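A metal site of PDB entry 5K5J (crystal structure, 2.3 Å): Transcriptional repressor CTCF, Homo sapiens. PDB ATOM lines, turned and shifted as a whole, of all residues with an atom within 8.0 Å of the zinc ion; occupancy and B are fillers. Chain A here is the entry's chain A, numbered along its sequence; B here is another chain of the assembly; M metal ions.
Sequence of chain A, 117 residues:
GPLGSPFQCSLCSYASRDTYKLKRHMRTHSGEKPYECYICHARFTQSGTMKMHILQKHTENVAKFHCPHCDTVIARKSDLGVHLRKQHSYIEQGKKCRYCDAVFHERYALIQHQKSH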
ATOM      1  N   GLN A   8      -9.933  -2.316  -8.697  1.00  0.00           N
ATOM      2  CA  GLN A   8     -10.647  -1.054  -8.692  1.00  0.00           C
ATOM      3  C   GLN A   8      -9.666   0.093  -8.464  1.00  0.00           C
ATOM      4  O   GLN A   8      -8.896   0.074  -7.499  1.00  0.00           O
ATOM      5  CB  GLN A   8     -11.715  -1.051  -7.597  1.00  0.00           C
ATOM      6  CG  GLN A   8     -12.597   0.174  -7.604  1.00  0.00           C
ATOM      7  CD  GLN A   8     -13.496   0.243  -8.810  1.00  0.00           C
ATOM      8  OE1 GLN A   8     -14.153  -0.729  -9.176  1.00  0.00           O
ATOM      9  NE2 GLN A   8     -13.523   1.410  -9.449  1.00  0.00           N
ATOM     10  N   CYS A   9      -9.696   1.084  -9.352  1.00  0.00           N
ATOM     11  CA  CYS A   9      -8.816   2.241  -9.220  1.00  0.00           C
ATOM     12  C   CYS A   9      -9.126   3.010  -7.949  1.00  0.00           C
ATOM     13  O   CYS A   9     -10.288   3.293  -7.645  1.00  0.00           O
ATOM     14  CB  CYS A   9      -8.947   3.160 -10.430  1.00  0.00           C
ATOM     15  SG  CYS A   9      -7.842   4.592 -10.332  1.00  0.00           S
ATOM     16  N   SER A  10      -8.080   3.350  -7.195  1.00  0.00           N
ATOM     17  CA  SER A  10      -8.229   4.031  -5.922  1.00  0.00           C
ATOM     18  C   SER A  10      -8.527   5.515  -6.062  1.00  0.00           C
ATOM     19  O   SER A  10      -8.774   6.185  -5.047  1.00  0.00           O
ATOM     20  CB  SER A  10      -6.971   3.844  -5.078  1.00  0.00           C
ATOM     21  OG  SER A  10      -5.829   4.390  -5.717  1.00  0.00           O
ATOM     22  N   LEU A  11      -8.512   6.061  -7.280  1.00  0.00           N
ATOM     23  CA  LEU A  11      -8.705   7.489  -7.510  1.00  0.00           C
ATOM     24  C   LEU A  11      -9.970   7.808  -8.284  1.00  0.00           C
ATOM     25  O   LEU A  11     -10.653   8.776  -7.944  1.00  0.00           O
ATOM     26  CB  LEU A  11      -7.488   8.058  -8.254  1.00  0.00           C
ATOM     27  CG  LEU A  11      -6.184   8.084  -7.457  1.00  0.00           C
ATOM     28  CD1 LEU A  11      -5.041   8.642  -8.301  1.00  0.00           C
ATOM     29  CD2 LEU A  11      -6.369   8.891  -6.178  1.00  0.00           C
ATOM     30  N   CYS A  12     -10.301   7.031  -9.311  1.00  0.00           N
ATOM     31  CA  CYS A  12     -11.485   7.272 -10.124  1.00  0.00           C
ATOM     32  C   CYS A  12     -12.342   6.011 -10.161  1.00  0.00           C
ATOM     33  O   CYS A  12     -12.107   5.072  -9.386  1.00  0.00           O
ATOM     34  CB  CYS A  12     -11.089   7.704 -11.537  1.00  0.00           C
ATOM     35  SG  CYS A  12     -10.603   6.362 -12.623  1.00  0.00           S
ATOM     36  N   SER A  13     -13.333   5.971 -11.038  1.00  0.00           N
ATOM     37  CA  SER A  13     -14.264   4.850 -11.111  1.00  0.00           C
ATOM     38  C   SER A  13     -13.796   3.730 -12.025  1.00  0.00           C
ATOM     39  O   SER A  13     -14.548   2.765 -12.226  1.00  0.00           O
ATOM     40  CB  SER A  13     -15.642   5.332 -11.561  1.00  0.00           C
ATOM     41  OG  SER A  13     -16.235   6.168 -10.577  1.00  0.00           O
ATOM     42  N   TYR A  14     -12.593   3.809 -12.582  1.00  0.00           N
ATOM     43  CA  TYR A  14     -12.127   2.772 -13.492  1.00  0.00           C
ATOM     44  C   TYR A  14     -11.863   1.470 -12.732  1.00  0.00           C
ATOM     45  O   TYR A  14     -11.469   1.465 -11.567  1.00  0.00           O
ATOM     46  CB  TYR A  14     -10.854   3.208 -14.221  1.00  0.00           C
ATOM     47  CG  TYR A  14     -10.313   2.165 -15.185  1.00  0.00           C
ATOM     48  CD1 TYR A  14     -10.894   1.978 -16.428  1.00  0.00           C
ATOM     49  CD2 TYR A  14      -9.221   1.374 -14.844  1.00  0.00           C
ATOM     50  CE1 TYR A  14     -10.401   1.018 -17.311  1.00  0.00           C
ATOM     51  CE2 TYR A  14      -8.722   0.422 -15.716  1.00  0.00           C
ATOM     52  CZ  TYR A  14      -9.309   0.252 -16.947  1.00  0.00           C
ATOM     53  OH  TYR A  14      -8.823  -0.690 -17.817  1.00  0.00           O
ATOM     54  N   ALA A  15     -12.096   0.352 -13.426  1.00  0.00           N
ATOM     55  CA  ALA A  15     -11.832  -0.966 -12.880  1.00  0.00           C
ATOM     56  C   ALA A  15     -11.438  -1.900 -14.017  1.00  0.00           C
ATOM     57  O   ALA A  15     -11.919  -1.759 -15.139  1.00  0.00           O
ATOM     58  CB  ALA A  15     -13.043  -1.529 -12.125  1.00  0.00           C
ATOM     59  N   LEU A  22      -4.751  -2.054 -14.944  1.00  0.00           N
ATOM     60  CA  LEU A  22      -4.883  -1.077 -13.874  1.00  0.00           C
ATOM     61  C   LEU A  22      -3.608  -0.260 -13.723  1.00  0.00           C
ATOM     62  O   LEU A  22      -3.659   0.955 -13.531  1.00  0.00           O
ATOM     63  CB  LEU A  22      -5.232  -1.766 -12.560  1.00  0.00           C
ATOM     64  CG  LEU A  22      -5.523  -0.795 -11.410  1.00  0.00           C
ATOM     65  CD1 LEU A  22      -6.587   0.212 -11.829  1.00  0.00           C
ATOM     66  CD2 LEU A  22      -5.945  -1.529 -10.154  1.00  0.00           C
ATOM     67  N   HIS A  25      -3.607   2.130 -16.587  1.00  0.00           N
ATOM     68  CA  HIS A  25      -4.557   3.204 -16.327  1.00  0.00           C
ATOM     69  C   HIS A  25      -4.013   4.208 -15.314  1.00  0.00           C
ATOM     70  O   HIS A  25      -4.300   5.400 -15.418  1.00  0.00           O
ATOM     71  CB  HIS A  25      -5.886   2.633 -15.840  1.00  0.00           C
ATOM     72  CG  HIS A  25      -6.760   3.648 -15.153  1.00  0.00           C
ATOM     73  ND1 HIS A  25      -7.449   4.615 -15.841  1.00  0.00           N
ATOM     74  CD2 HIS A  25      -7.026   3.851 -13.848  1.00  0.00           C
ATOM     75  CE1 HIS A  25      -8.113   5.374 -14.992  1.00  0.00           C
ATOM     76  NE2 HIS A  25      -7.880   4.922 -13.766  1.00  0.00           N
ATOM     77  N   MET A  26      -3.236   3.734 -14.336  1.00  0.00           N
ATOM     78  CA  MET A  26      -2.692   4.622 -13.321  1.00  0.00           C
ATOM     79  C   MET A  26      -1.759   5.671 -13.910  1.00  0.00           C
ATOM     80  O   MET A  26      -1.544   6.711 -13.287  1.00  0.00           O
ATOM     81  CB  MET A  26      -1.958   3.822 -12.249  1.00  0.00           C
ATOM     82  CG  MET A  26      -2.872   3.056 -11.308  1.00  0.00           C
ATOM     83  SD  MET A  26      -4.087   4.113 -10.483  1.00  0.00           S
ATOM     84  CE  MET A  26      -4.727   2.996  -9.241  1.00  0.00           C
ATOM     85  N   ARG A  27      -1.196   5.423 -15.098  1.00  0.00           N
ATOM     86  CA  ARG A  27      -0.375   6.424 -15.757  1.00  0.00           C
ATOM     87  C   ARG A  27      -1.175   7.666 -16.130  1.00  0.00           C
ATOM     88  O   ARG A  27      -0.602   8.741 -16.275  1.00  0.00           O
ATOM     89  CB  ARG A  27       0.282   5.832 -17.008  1.00  0.00           C
ATOM     90  CG  ARG A  27       1.222   4.678 -16.728  1.00  0.00           C
ATOM     91  CD  ARG A  27       1.720   4.087 -18.030  1.00  0.00           C
ATOM     92  NE  ARG A  27       2.231   2.725 -17.862  1.00  0.00           N
ATOM     93  CZ  ARG A  27       2.321   1.840 -18.840  1.00  0.00           C
ATOM     94  NH1 ARG A  27       1.932   2.172 -20.065  1.00  0.00           N
ATOM     95  NH2 ARG A  27       2.792   0.624 -18.607  1.00  0.00           N
ATOM     96  N   THR A  28      -2.497   7.530 -16.294  1.00  0.00           N
ATOM     97  CA  THR A  28      -3.329   8.695 -16.545  1.00  0.00           C
ATOM     98  C   THR A  28      -3.436   9.599 -15.325  1.00  0.00           C
ATOM     99  O   THR A  28      -3.747  10.783 -15.456  1.00  0.00           O
ATOM    100  CB  THR A  28      -4.734   8.273 -16.985  1.00  0.00           C
ATOM    101  OG1 THR A  28      -5.447   7.727 -15.860  1.00  0.00           O
ATOM    102  CG2 THR A  28      -4.651   7.217 -18.077  1.00  0.00           C
ATOM    103  N   HIS A  29      -3.175   9.064 -14.130  1.00  0.00           N
ATOM    104  CA  HIS A  29      -3.219   9.846 -12.898  1.00  0.00           C
ATOM    105  C   HIS A  29      -1.829  10.368 -12.525  1.00  0.00           C
ATOM    106  O   HIS A  29      -1.677  11.539 -12.164  1.00  0.00           O
ATOM    107  CB  HIS A  29      -3.792   9.010 -11.755  1.00  0.00           C
ATOM    108  CG  HIS A  29      -5.200   8.546 -12.000  1.00  0.00           C
ATOM    109  ND1 HIS A  29      -6.272   9.410 -12.034  1.00  0.00           N
ATOM    110  CD2 HIS A  29      -5.697   7.302 -12.199  1.00  0.00           C
ATOM    111  CE1 HIS A  29      -7.377   8.716 -12.264  1.00  0.00           C
ATOM    112  NE2 HIS A  29      -7.052   7.440 -12.361  1.00  0.00           N
ATOM    113  P    DA B   9      -7.482   4.854 -19.519  1.00  0.00           P
ATOM    114  OP1  DA B   9      -8.197   5.199 -18.277  1.00  0.00           O
ATOM    115  OP2  DA B   9      -6.084   4.384 -19.443  1.00  0.00           O
ATOM    116  O5'  DA B   9      -8.334   3.744 -20.297  1.00  0.00           O
ATOM    117  C5'  DA B   9      -9.601   4.075 -20.844  1.00  0.00           C
ATOM    118  C4'  DA B   9     -10.131   2.953 -21.700  1.00  0.00           C
ATOM    119  O4'  DA B   9      -9.352   2.862 -22.923  1.00  0.00           O
ATOM    120  C3'  DA B   9     -10.083   1.564 -21.069  1.00  0.00           C
ATOM    121  O3'  DA B   9     -11.255   0.842 -21.411  1.00  0.00           O
ATOM    122  C2'  DA B   9      -8.827   0.955 -21.690  1.00  0.00           C
ATOM    123  C1'  DA B   9      -8.871   1.554 -23.083  1.00  0.00           C
ATOM    124  N9   DA B   9      -7.554   1.618 -23.724  1.00  0.00           N
ATOM    125  C8   DA B   9      -6.387   2.071 -23.177  1.00  0.00           C
ATOM    126  N7   DA B   9      -5.364   2.011 -23.988  1.00  0.00           N
ATOM    127  C5   DA B   9      -5.889   1.495 -25.152  1.00  0.00           C
ATOM    128  C6   DA B   9      -5.316   1.176 -26.405  1.00  0.00           C
ATOM    129  N6   DA B   9      -4.025   1.368 -26.689  1.00  0.00           N
ATOM    130  N1   DA B   9      -6.124   0.671 -27.360  1.00  0.00           N
ATOM    131  C2   DA B   9      -7.418   0.484 -27.068  1.00  0.00           C
ATOM    132  N3   DA B   9      -8.076   0.731 -25.934  1.00  0.00           N
ATOM    133  C4   DA B   9      -7.244   1.237 -25.006  1.00  0.00           C
HETATM  134 ZN    ZN M   1      -8.408   5.989 -12.086  1.00  0.00          ZN
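Of the 15 residues printed, 4 come within 4 Å of the zinc ion.
O of His 25 lies within hydrogen-bond range of OG1 of Thr 28 (2.6 Å).
A ring nitrogen (ND1) of His 25 sits at hydrogen-bond distance from OP1 of DA 9 of chain B.
SG of Cys 12 lies close to N of Tyr 14, 3.2 Å away.
The backbone NH of Cys 9 of chain A sits at hydrogen-bond distance from the backbone carbonyl oxygen of Tyr 14.
The backbone NH (N) of Leu 11 lies close to the side-chain sulfur (SG) of Cys 9 of chain A (3.5 Å).
The side-chain sulfur (SG) of Cys 9 of chain A lies close to the side-chain sulfur (SD) of Met 26, 3.8 Å away.
The zinc ion is bound by NE2 of His 29 (2.0 Å), NE2 of His 25 (2.1 Å), SG of Cys 12 (2.3 Å) and SG of Cys 9 of chain A (2.3 Å).
The zinc ion has four donor atoms within binding distance.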
